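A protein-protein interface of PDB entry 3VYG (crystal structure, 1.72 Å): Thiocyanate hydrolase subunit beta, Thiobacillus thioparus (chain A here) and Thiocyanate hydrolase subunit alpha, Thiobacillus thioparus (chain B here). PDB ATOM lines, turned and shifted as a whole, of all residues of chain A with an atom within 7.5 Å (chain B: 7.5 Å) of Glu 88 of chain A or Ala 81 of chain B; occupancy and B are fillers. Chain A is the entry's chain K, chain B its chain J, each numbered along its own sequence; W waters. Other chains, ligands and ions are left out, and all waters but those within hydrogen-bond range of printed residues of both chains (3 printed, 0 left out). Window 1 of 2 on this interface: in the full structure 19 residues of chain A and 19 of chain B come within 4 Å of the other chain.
The side-chain carboxylate (OE1) of Glu 88 of chain A is in salt-bridge range of the guanidinium group (NE) of Arg 55 of chain B, at 3.5 Å. The guanidinium group (NE) of Arg 92 of chain A sits at hydrogen-bond distance from the backbone carbonyl oxygen (O) of Ala 81 of chain B (3.0 Å). OE2 of Glu 88 of chain A sits at hydrogen-bond distance from OH of Tyr 53 of chain B, at 2.6 Å. O of Thr 54 of chain B is in hydrogen-bond range of NE2 of His 48 of chain A, at 3.0 Å.
The side-chain hydroxyl of Thr 54 of chain B sits at hydrogen-bond distance from the side-chain carboxylate of Glu 78 of chain B, at 3.1 Å. NH1 of Arg 91 of chain A lies within salt-bridge range of OE1 of Glu 88 of chain A (3.0 Å). The backbone NH (N) of Arg 55 of chain B sits at hydrogen-bond distance from the side-chain carboxylate (OE2) of Glu 78 of chain B (3.4 Å). The side-chain carboxylate (OD2) of Asp 97 of chain A is in salt-bridge range of the guanidinium group (NH1) of Arg 92 of chain A, 2.9 Å away. N of Thr 86 of chain A lies within hydrogen-bond range of OE1 of Glu 89 of chain A (3.0 Å). The side-chain hydroxyl of Tyr 53 of chain B sits at hydrogen-bond distance from the guanidinium group of Arg 55 of chain B (2.8 Å).
CE1 of Tyr 53 of chain B touches CE1 of His 48 of chain A, 3.6 Å away. O of Glu 80 of chain B touches OG1 of Thr 86 of chain A, at 3.9 Å. Thr 86 of chain A touches Glu 85 of chain B. Glu 88 of chain A touches Ala 77 of chain B. Glu 80 of chain B touches Glu 88 of chain A. O of Glu 88 of chain A touches CB of Ala 81 of chain B, 3.4 Å away. Ala 81 of chain B touches Glu 89 of chain A. OE2 of Glu 89 of chain A touches CA of Gly 83 of chain B, at 3.97 Å. NH1 of Arg 55 of chain B touches CD of Arg 91 of chain A, 3.4 Å away. Arg 92 of chain A touches Phe 82 of chain B.
Of chain A, only Glu 88, Glu 89 and Arg 92 come within 4 Å of Ala 81 of chain B. Ala 87 of chain A touches none of the printed residues of chain B. Of the printed residues of chain A, Gly 83 of chain B touches Glu 89 (3.97 Å). Of the printed residues of chain A, Thr 54 of chain B touches His 48. Of the printed residues of chain B, His 48 of chain A touches Tyr 53, Thr 54 and Arg 55. Of the printed residues of chain A, Arg 55 of chain B touches His 48, Glu 88 and Arg 91. The nearest residue of chain B that does not touch Glu 88 of chain A is Glu 78 of chain B (5.6 Å). The nearest residue of chain A that does not touch Ala 81 of chain B is Thr 86 of chain A (5.3 Å).
Of the 14 printed residues of chain A, 6 touch a printed residue of chain B. Printed residues of chain A that touch a printed residue of chain B: His 48, Thr 86, Glu 88, Glu 89, Arg 91 and Arg 92. Hydrophobic or aromatic side chains of chain A that line the printed part of chain B: His 48. Along chain A the printed residues that touch a printed residue of chain B span positions 48 to 92. Of the 15 printed residues of chain B, 9 touch a printed residue of chain A. Printed residues of chain B that touch a printed residue of chain A: Tyr 53, Thr 54, Arg 55, Ala 77, Glu 80, Ala 81, Phe 82, Gly 83 and Glu 85.
Water W2 lies within hydrogen-bond range of OE2 of Glu 85 of chain B (2.7 Å), O of Glu 80 of chain B (2.8 Å) and OG1 of Thr 86 of chain A (2.9 Å). Water W1 lies within hydrogen-bond range of a ring nitrogen (ND1) of His 48 of chain A, the side-chain amide nitrogen (ND2) of Asn 95 of chain A and the guanidinium group (NH1) of Arg 55 of chain B. Water W3 bridges the side-chain carboxylate (OE1) of Glu 80 of chain B (3.1 Å) and the backbone NH (N) of Glu 88 of chain A (3.2 Å).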
ATOM      1  N   HIS A  48     -28.247  13.935 -28.928  1.00  0.00           N
ATOM      2  CA  HIS A  48     -28.647  14.784 -27.815  1.00  0.00           C
ATOM      3  C   HIS A  48     -28.284  16.254 -27.992  1.00  0.00           C
ATOM      4  O   HIS A  48     -28.748  17.122 -27.233  1.00  0.00           O
ATOM      5  CB  HIS A  48     -28.063  14.217 -26.469  1.00  0.00           C
ATOM      6  CG  HIS A  48     -26.540  14.351 -26.303  1.00  0.00           C
ATOM      7  ND1 HIS A  48     -25.930  14.021 -25.104  1.00  0.00           N
ATOM      8  CD2 HIS A  48     -25.538  14.662 -27.152  1.00  0.00           C
ATOM      9  CE1 HIS A  48     -24.604  14.186 -25.191  1.00  0.00           C
ATOM     10  NE2 HIS A  48     -24.329  14.599 -26.426  1.00  0.00           N
ATOM     11  N   ALA A  80     -26.858   2.814 -10.586  1.00  0.00           N
ATOM     12  CA  ALA A  80     -25.656   3.589 -10.491  1.00  0.00           C
ATOM     13  C   ALA A  80     -25.105   3.574  -9.042  1.00  0.00           C
ATOM     14  O   ALA A  80     -23.926   3.375  -8.841  1.00  0.00           O
ATOM     15  CB  ALA A  80     -25.877   5.101 -11.014  1.00  0.00           C
ATOM     16  N   TRP A  85     -23.366   0.980 -13.422  1.00  0.00           N
ATOM     17  CA  TRP A  85     -22.857   2.029 -14.294  1.00  0.00           C
ATOM     18  C   TRP A  85     -22.699   3.356 -13.551  1.00  0.00           C
ATOM     19  O   TRP A  85     -23.124   3.470 -12.413  1.00  0.00           O
ATOM     20  CB  TRP A  85     -23.807   2.247 -15.486  1.00  0.00           C
ATOM     21  CG  TRP A  85     -25.277   2.520 -15.189  1.00  0.00           C
ATOM     22  CD1 TRP A  85     -25.870   2.827 -13.961  1.00  0.00           C
ATOM     23  CD2 TRP A  85     -26.295   2.592 -16.164  1.00  0.00           C
ATOM     24  NE1 TRP A  85     -27.245   3.026 -14.131  1.00  0.00           N
ATOM     25  CE2 TRP A  85     -27.524   2.934 -15.489  1.00  0.00           C
ATOM     26  CE3 TRP A  85     -26.291   2.469 -17.607  1.00  0.00           C
ATOM     27  CZ2 TRP A  85     -28.747   3.028 -16.149  1.00  0.00           C
ATOM     28  CZ3 TRP A  85     -27.544   2.586 -18.306  1.00  0.00           C
ATOM     29  CH2 TRP A  85     -28.772   2.879 -17.557  1.00  0.00           C
ATOM     30  N   THR A  86     -22.124   4.330 -14.227  1.00  0.00           N
ATOM     31  CA  THR A  86     -22.136   5.767 -13.792  1.00  0.00           C
ATOM     32  C   THR A  86     -23.175   6.502 -14.638  1.00  0.00           C
ATOM     33  O   THR A  86     -23.622   5.968 -15.677  1.00  0.00           O
ATOM     34  CB  THR A  86     -20.772   6.478 -14.012  1.00  0.00           C
ATOM     35  OG1 THR A  86     -20.389   6.385 -15.406  1.00  0.00           O
ATOM     36  CG2 THR A  86     -19.584   5.816 -13.088  1.00  0.00           C
ATOM     37  N   ALA A  87     -23.596   7.706 -14.187  1.00  0.00           N
ATOM     38  CA  ALA A  87     -24.665   8.389 -14.921  1.00  0.00           C
ATOM     39  C   ALA A  87     -24.090   8.777 -16.294  1.00  0.00           C
ATOM     40  O   ALA A  87     -24.856   8.842 -17.268  1.00  0.00           O
ATOM     41  CB  ALA A  87     -25.060   9.605 -14.196  1.00  0.00           C
ATOM     42  N   GLU A  88     -22.781   9.066 -16.417  1.00  0.00           N
ATOM     43  CA  GLU A  88     -22.295   9.367 -17.785  1.00  0.00           C
ATOM     44  C   GLU A  88     -22.361   8.229 -18.764  1.00  0.00           C
ATOM     45  O   GLU A  88     -22.773   8.446 -19.962  1.00  0.00           O
ATOM     46  CB  GLU A  88     -20.840   9.869 -17.740  1.00  0.00           C
ATOM     47  CG  GLU A  88     -20.877  11.460 -17.522  1.00  0.00           C
ATOM     48  CD  GLU A  88     -21.545  12.149 -18.737  1.00  0.00           C
ATOM     49  OE1 GLU A  88     -22.459  12.965 -18.558  1.00  0.00           O
ATOM     50  OE2 GLU A  88     -21.227  11.687 -19.868  1.00  0.00           O
ATOM     51  N   GLU A  89     -22.127   7.024 -18.247  1.00  0.00           N
ATOM     52  CA  GLU A  89     -22.366   5.823 -19.065  1.00  0.00           C
ATOM     53  C   GLU A  89     -23.837   5.789 -19.451  1.00  0.00           C
ATOM     54  O   GLU A  89     -24.142   5.543 -20.637  1.00  0.00           O
ATOM     55  CB  GLU A  89     -21.970   4.515 -18.358  1.00  0.00           C
ATOM     56  CG  GLU A  89     -20.501   4.409 -18.167  1.00  0.00           C
ATOM     57  CD  GLU A  89     -20.076   3.093 -17.445  1.00  0.00           C
ATOM     58  OE1 GLU A  89     -20.368   3.040 -16.257  1.00  0.00           O
ATOM     59  OE2 GLU A  89     -19.508   2.120 -18.027  1.00  0.00           O
ATOM     60  N   ARG A  90     -24.766   5.929 -18.507  1.00  0.00           N
ATOM     61  CA  ARG A  90     -26.199   6.002 -18.858  1.00  0.00           C
ATOM     62  C   ARG A  90     -26.478   7.080 -19.937  1.00  0.00           C
ATOM     63  O   ARG A  90     -27.193   6.762 -20.909  1.00  0.00           O
ATOM     64  CB  ARG A  90     -27.041   6.298 -17.627  1.00  0.00           C
ATOM     65  CG  ARG A  90     -28.518   6.419 -17.943  1.00  0.00           C
ATOM     66  CD  ARG A  90     -29.374   6.616 -16.618  1.00  0.00           C
ATOM     67  NE  ARG A  90     -29.031   7.895 -15.953  1.00  0.00           N
ATOM     68  CZ  ARG A  90     -29.287   9.104 -16.424  1.00  0.00           C
ATOM     69  NH1 ARG A  90     -29.931   9.321 -17.628  1.00  0.00           N
ATOM     70  NH2 ARG A  90     -28.913  10.150 -15.670  1.00  0.00           N
ATOM     71  N   ARG A  91     -25.946   8.293 -19.768  1.00  0.00           N
ATOM     72  CA  ARG A  91     -26.346   9.373 -20.717  1.00  0.00           C
ATOM     73  C   ARG A  91     -25.909   9.015 -22.125  1.00  0.00           C
ATOM     74  O   ARG A  91     -26.623   9.221 -23.087  1.00  0.00           O
ATOM     75  CB  ARG A  91     -25.711  10.718 -20.329  1.00  0.00           C
ATOM     76  CG  ARG A  91     -26.403  11.321 -19.065  1.00  0.00           C
ATOM     77  CD  ARG A  91     -25.893  12.776 -18.883  1.00  0.00           C
ATOM     78  NE  ARG A  91     -26.385  13.205 -17.566  1.00  0.00           N
ATOM     79  CZ  ARG A  91     -25.713  12.960 -16.425  1.00  0.00           C
ATOM     80  NH1 ARG A  91     -24.454  12.395 -16.426  1.00  0.00           N
ATOM     81  NH2 ARG A  91     -26.356  13.246 -15.266  1.00  0.00           N
ATOM     82  N   ARG A  92     -24.694   8.495 -22.243  1.00  0.00           N
ATOM     83  CA  ARG A  92     -24.185   8.166 -23.519  1.00  0.00           C
ATOM     84  C   ARG A  92     -24.994   7.046 -24.155  1.00  0.00           C
ATOM     85  O   ARG A  92     -25.334   7.162 -25.360  1.00  0.00           O
ATOM     86  CB  ARG A  92     -22.693   7.774 -23.384  1.00  0.00           C
ATOM     87  CG  ARG A  92     -21.994   7.270 -24.733  1.00  0.00           C
ATOM     88  CD  ARG A  92     -22.096   5.724 -24.826  1.00  0.00           C
ATOM     89  NE  ARG A  92     -21.401   4.957 -23.714  1.00  0.00           N
ATOM     90  CZ  ARG A  92     -21.362   3.616 -23.707  1.00  0.00           C
ATOM     91  NH1 ARG A  92     -21.983   2.850 -24.707  1.00  0.00           N
ATOM     92  NH2 ARG A  92     -20.686   2.940 -22.757  1.00  0.00           N
ATOM     93  N   LYS A  93     -25.357   5.996 -23.373  1.00  0.00           N
ATOM     94  CA  LYS A  93     -26.256   4.929 -23.965  1.00  0.00           C
ATOM     95  C   LYS A  93     -27.687   5.434 -24.262  1.00  0.00           C
ATOM     96  O   LYS A  93     -28.282   5.067 -25.278  1.00  0.00           O
ATOM     97  CB  LYS A  93     -26.385   3.761 -22.966  1.00  0.00           C
ATOM     98  CG  LYS A  93     -25.006   3.136 -22.736  1.00  0.00           C
ATOM     99  CD  LYS A  93     -25.187   1.978 -21.705  1.00  0.00           C
ATOM    100  CE  LYS A  93     -25.814   0.709 -22.319  1.00  0.00           C
ATOM    101  NZ  LYS A  93     -24.882   0.170 -23.402  1.00  0.00           N
ATOM    102  N   GLN A  94     -28.228   6.253 -23.371  1.00  0.00           N
ATOM    103  CA  GLN A  94     -29.669   6.597 -23.405  1.00  0.00           C
ATOM    104  C   GLN A  94     -29.975   7.740 -24.383  1.00  0.00           C
ATOM    105  O   GLN A  94     -31.085   7.808 -25.013  1.00  0.00           O
ATOM    106  CB  GLN A  94     -29.934   7.115 -22.010  1.00  0.00           C
ATOM    107  CG  GLN A  94     -31.371   7.544 -21.799  1.00  0.00           C
ATOM    108  CD  GLN A  94     -31.533   8.166 -20.401  1.00  0.00           C
ATOM    109  OE1 GLN A  94     -31.321   7.475 -19.414  1.00  0.00           O
ATOM    110  NE2 GLN A  94     -31.795   9.480 -20.358  1.00  0.00           N
ATOM    111  N   ASN A  95     -29.041   8.703 -24.486  1.00  0.00           N
ATOM    112  CA  ASN A  95     -29.348   9.955 -25.214  1.00  0.00           C
ATOM    113  C   ASN A  95     -28.605  10.007 -26.508  1.00  0.00           C
ATOM    114  O   ASN A  95     -28.835  10.922 -27.336  1.00  0.00           O
ATOM    115  CB  ASN A  95     -28.973  11.199 -24.340  1.00  0.00           C
ATOM    116  CG  ASN A  95     -29.694  11.174 -23.012  1.00  0.00           C
ATOM    117  OD1 ASN A  95     -30.829  10.698 -22.903  1.00  0.00           O
ATOM    118  ND2 ASN A  95     -29.095  11.747 -21.975  1.00  0.00           N
ATOM    119  N   ASP A  97     -26.542   6.635 -28.022  1.00  0.00           N
ATOM    120  CA  ASP A  97     -26.443   5.353 -28.698  1.00  0.00           C
ATOM    121  C   ASP A  97     -27.813   4.877 -29.261  1.00  0.00           C
ATOM    122  O   ASP A  97     -27.809   4.106 -30.231  1.00  0.00           O
ATOM    123  CB  ASP A  97     -25.951   4.224 -27.756  1.00  0.00           C
ATOM    124  CG  ASP A  97     -24.497   4.369 -27.368  1.00  0.00           C
ATOM    125  OD1 ASP A  97     -23.758   5.259 -27.920  1.00  0.00           O
ATOM    126  OD2 ASP A  97     -24.097   3.507 -26.511  1.00  0.00           O
ATOM    127  N   TYR B  53     -19.386  10.177 -28.954  1.00  0.00           N
ATOM    128  CA  TYR B  53     -19.859  10.905 -27.762  1.00  0.00           C
ATOM    129  C   TYR B  53     -19.059  12.178 -27.556  1.00  0.00           C
ATOM    130  O   TYR B  53     -17.865  12.239 -27.855  1.00  0.00           O
ATOM    131  CB  TYR B  53     -19.669  10.023 -26.485  1.00  0.00           C
ATOM    132  CG  TYR B  53     -20.444  10.584 -25.310  1.00  0.00           C
ATOM    133  CD1 TYR B  53     -21.846  10.782 -25.378  1.00  0.00           C
ATOM    134  CD2 TYR B  53     -19.833  10.895 -24.109  1.00  0.00           C
ATOM    135  CE1 TYR B  53     -22.608  11.296 -24.250  1.00  0.00           C
ATOM    136  CE2 TYR B  53     -20.567  11.424 -22.989  1.00  0.00           C
ATOM    137  CZ  TYR B  53     -21.925  11.592 -23.061  1.00  0.00           C
ATOM    138  OH  TYR B  53     -22.647  12.041 -21.970  1.00  0.00           O
ATOM    139  N   THR B  54     -19.778  13.230 -27.124  1.00  0.00           N
ATOM    140  CA  THR B  54     -19.122  14.460 -26.667  1.00  0.00           C
ATOM    141  C   THR B  54     -20.131  15.195 -25.812  1.00  0.00           C
ATOM    142  O   THR B  54     -21.363  15.059 -26.021  1.00  0.00           O
ATOM    143  CB  THR B  54     -18.649  15.419 -27.821  1.00  0.00           C
ATOM    144  OG1 THR B  54     -18.083  16.573 -27.195  1.00  0.00           O
ATOM    145  CG2 THR B  54     -19.794  15.909 -28.628  1.00  0.00           C
ATOM    146  N   ARG B  55     -19.641  15.972 -24.851  1.00  0.00           N
ATOM    147  CA  ARG B  55     -20.588  16.926 -24.161  1.00  0.00           C
ATOM    148  C   ARG B  55     -20.164  18.367 -24.415  1.00  0.00           C
ATOM    149  O   ARG B  55     -20.569  19.294 -23.686  1.00  0.00           O
ATOM    150  CB  ARG B  55     -20.626  16.653 -22.604  1.00  0.00           C
ATOM    151  CG  ARG B  55     -21.259  15.252 -22.370  1.00  0.00           C
ATOM    152  CD  ARG B  55     -21.593  15.119 -20.856  1.00  0.00           C
ATOM    153  NE  ARG B  55     -22.803  15.829 -20.456  1.00  0.00           N
ATOM    154  CZ  ARG B  55     -24.057  15.440 -20.746  1.00  0.00           C
ATOM    155  NH1 ARG B  55     -24.282  14.261 -21.458  1.00  0.00           N
ATOM    156  NH2 ARG B  55     -25.047  16.229 -20.314  1.00  0.00           N
ATOM    157  N   SER B  74     -12.150  16.488 -13.102  1.00  0.00           N
ATOM    158  CA  SER B  74     -12.945  15.289 -13.329  1.00  0.00           C
ATOM    159  C   SER B  74     -12.355  14.570 -14.585  1.00  0.00           C
ATOM    160  O   SER B  74     -11.780  15.243 -15.416  1.00  0.00           O
ATOM    161  CB  SER B  74     -14.396  15.703 -13.580  1.00  0.00           C
ATOM    162  OG  SER B  74     -15.229  14.614 -13.963  1.00  0.00           O
ATOM    163  N   PRO B  75     -12.544  13.246 -14.728  1.00  0.00           N
ATOM    164  CA  PRO B  75     -12.362  12.663 -16.075  1.00  0.00           C
ATOM    165  C   PRO B  75     -13.301  13.371 -17.063  1.00  0.00           C
ATOM    166  O   PRO B  75     -14.355  13.848 -16.653  1.00  0.00           O
ATOM    167  CB  PRO B  75     -12.898  11.206 -15.934  1.00  0.00           C
ATOM    168  CG  PRO B  75     -12.693  10.907 -14.397  1.00  0.00           C
ATOM    169  CD  PRO B  75     -13.006  12.235 -13.742  1.00  0.00           C
ATOM    170  N   ALA B  76     -12.867  13.508 -18.301  1.00  0.00           N
ATOM    171  CA  ALA B  76     -13.760  14.073 -19.306  1.00  0.00           C
ATOM    172  C   ALA B  76     -14.942  13.128 -19.497  1.00  0.00           C
ATOM    173  O   ALA B  76     -14.754  11.897 -19.383  1.00  0.00           O
ATOM    174  CB  ALA B  76     -12.988  14.156 -20.585  1.00  0.00           C
ATOM    175  N   ALA B  77     -16.119  13.668 -19.886  1.00  0.00           N
ATOM    176  CA  ALA B  77     -17.237  12.756 -20.065  1.00  0.00           C
ATOM    177  C   ALA B  77     -16.894  11.799 -21.212  1.00  0.00           C
ATOM    178  O   ALA B  77     -17.471  10.656 -21.231  1.00  0.00           O
ATOM    179  CB  ALA B  77     -18.573  13.584 -20.414  1.00  0.00           C
ATOM    180  N   GLU B  78     -16.191  12.219 -22.275  1.00  0.00           N
ATOM    181  CA  GLU B  78     -15.822  11.296 -23.348  1.00  0.00           C
ATOM    182  C   GLU B  78     -15.103  10.033 -22.882  1.00  0.00           C
ATOM    183  O   GLU B  78     -15.183   8.993 -23.481  1.00  0.00           O
ATOM    184  CB  GLU B  78     -14.849  12.013 -24.359  1.00  0.00           C
ATOM    185  CG  GLU B  78     -15.587  13.212 -25.088  1.00  0.00           C
ATOM    186  CD  GLU B  78     -15.724  14.507 -24.334  1.00  0.00           C
ATOM    187  OE1 GLU B  78     -15.400  14.640 -23.151  1.00  0.00           O
ATOM    188  OE2 GLU B  78     -16.308  15.477 -24.880  1.00  0.00           O
ATOM    189  N   ASP B  79     -14.471  10.147 -21.715  1.00  0.00           N
ATOM    190  CA  ASP B  79     -13.841   8.983 -21.091  1.00  0.00           C
ATOM    191  C   ASP B  79     -14.731   8.364 -20.031  1.00  0.00           C
ATOM    192  O   ASP B  79     -14.932   7.146 -20.075  1.00  0.00           O
ATOM    193  CB  ASP B  79     -12.524   9.390 -20.435  1.00  0.00           C
ATOM    194  CG  ASP B  79     -11.408   9.617 -21.509  1.00  0.00           C
ATOM    195  OD1 ASP B  79     -11.405   8.953 -22.568  1.00  0.00           O
ATOM    196  OD2 ASP B  79     -10.584  10.512 -21.257  1.00  0.00           O
ATOM    197  N   GLU B  80     -15.333   9.167 -19.172  1.00  0.00           N
ATOM    198  CA  GLU B  80     -16.152   8.548 -18.109  1.00  0.00           C
ATOM    199  C   GLU B  80     -17.314   7.719 -18.734  1.00  0.00           C
ATOM    200  O   GLU B  80     -17.687   6.674 -18.225  1.00  0.00           O
ATOM    201  CB  GLU B  80     -16.761   9.662 -17.261  1.00  0.00           C
ATOM    202  CG  GLU B  80     -17.149   9.249 -15.896  1.00  0.00           C
ATOM    203  CD  GLU B  80     -17.362  10.489 -15.000  1.00  0.00           C
ATOM    204  OE1 GLU B  80     -18.083  11.394 -15.443  1.00  0.00           O
ATOM    205  OE2 GLU B  80     -16.731  10.624 -13.889  1.00  0.00           O
ATOM    206  N   ALA B  81     -17.913   8.197 -19.847  1.00  0.00           N
ATOM    207  CA  ALA B  81     -19.061   7.441 -20.402  1.00  0.00           C
ATOM    208  C   ALA B  81     -18.705   6.115 -21.051  1.00  0.00           C
ATOM    209  O   ALA B  81     -19.586   5.360 -21.387  1.00  0.00           O
ATOM    210  CB  ALA B  81     -19.745   8.384 -21.458  1.00  0.00           C
ATOM    211  N   PHE B  82     -17.423   5.791 -21.177  1.00  0.00           N
ATOM    212  CA  PHE B  82     -17.001   4.472 -21.675  1.00  0.00           C
ATOM    213  C   PHE B  82     -16.205   3.741 -20.590  1.00  0.00           C
ATOM    214  O   PHE B  82     -15.597   2.734 -20.891  1.00  0.00           O
ATOM    215  CB  PHE B  82     -16.190   4.617 -22.948  1.00  0.00           C
ATOM    216  CG  PHE B  82     -17.087   5.014 -24.122  1.00  0.00           C
ATOM    217  CD1 PHE B  82     -17.785   4.016 -24.783  1.00  0.00           C
ATOM    218  CD2 PHE B  82     -17.274   6.350 -24.436  1.00  0.00           C
ATOM    219  CE1 PHE B  82     -18.644   4.368 -25.870  1.00  0.00           C
ATOM    220  CE2 PHE B  82     -18.151   6.733 -25.461  1.00  0.00           C
ATOM    221  CZ  PHE B  82     -18.807   5.744 -26.157  1.00  0.00           C
ATOM    222  N   GLY B  83     -16.353   4.235 -19.340  1.00  0.00           N
ATOM    223  CA  GLY B  83     -15.790   3.515 -18.171  1.00  0.00           C
ATOM    224  C   GLY B  83     -14.311   3.776 -17.981  1.00  0.00           C
ATOM    225  O   GLY B  83     -13.652   2.940 -17.309  1.00  0.00           O
ATOM    226  N   ASN B  84     -13.767   4.882 -18.506  1.00  0.00           N
ATOM    227  CA  ASN B  84     -12.284   5.176 -18.480  1.00  0.00           C
ATOM    228  C   ASN B  84     -12.066   6.346 -17.583  1.00  0.00           C
ATOM    229  O   ASN B  84     -12.423   7.474 -17.939  1.00  0.00           O
ATOM    230  CB  ASN B  84     -11.771   5.453 -19.891  1.00  0.00           C
ATOM    231  CG  ASN B  84     -12.068   4.306 -20.845  1.00  0.00           C
ATOM    232  OD1 ASN B  84     -12.575   4.516 -22.017  1.00  0.00           O
ATOM    233  ND2 ASN B  84     -11.747   3.090 -20.427  1.00  0.00           N
ATOM    234  N   GLU B  85     -11.552   6.069 -16.351  1.00  0.00           N
ATOM    235  CA  GLU B  85     -11.507   7.238 -15.476  1.00  0.00           C
ATOM    236  C   GLU B  85     -10.083   7.471 -14.984  1.00  0.00           C
ATOM    237  O   GLU B  85      -9.896   8.211 -13.987  1.00  0.00           O
ATOM    238  CB  GLU B  85     -12.393   6.990 -14.242  1.00  0.00           C
ATOM    239  CG  GLU B  85     -13.911   6.917 -14.511  1.00  0.00           C
ATOM    240  CD  GLU B  85     -14.750   6.584 -13.320  1.00  0.00           C
ATOM    241  OE1 GLU B  85     -14.196   6.508 -12.177  1.00  0.00           O
ATOM    242  OE2 GLU B  85     -15.994   6.410 -13.540  1.00  0.00           O
HETATM  243  O   HOH W   1     -26.975  13.682 -22.475  1.00  0.00           O
HETATM  244  O   HOH W   2     -17.548   5.664 -15.598  1.00  0.00           O
HETATM  245  O   HOH W   3     -20.774  10.246 -14.276  1.00  0.00           O
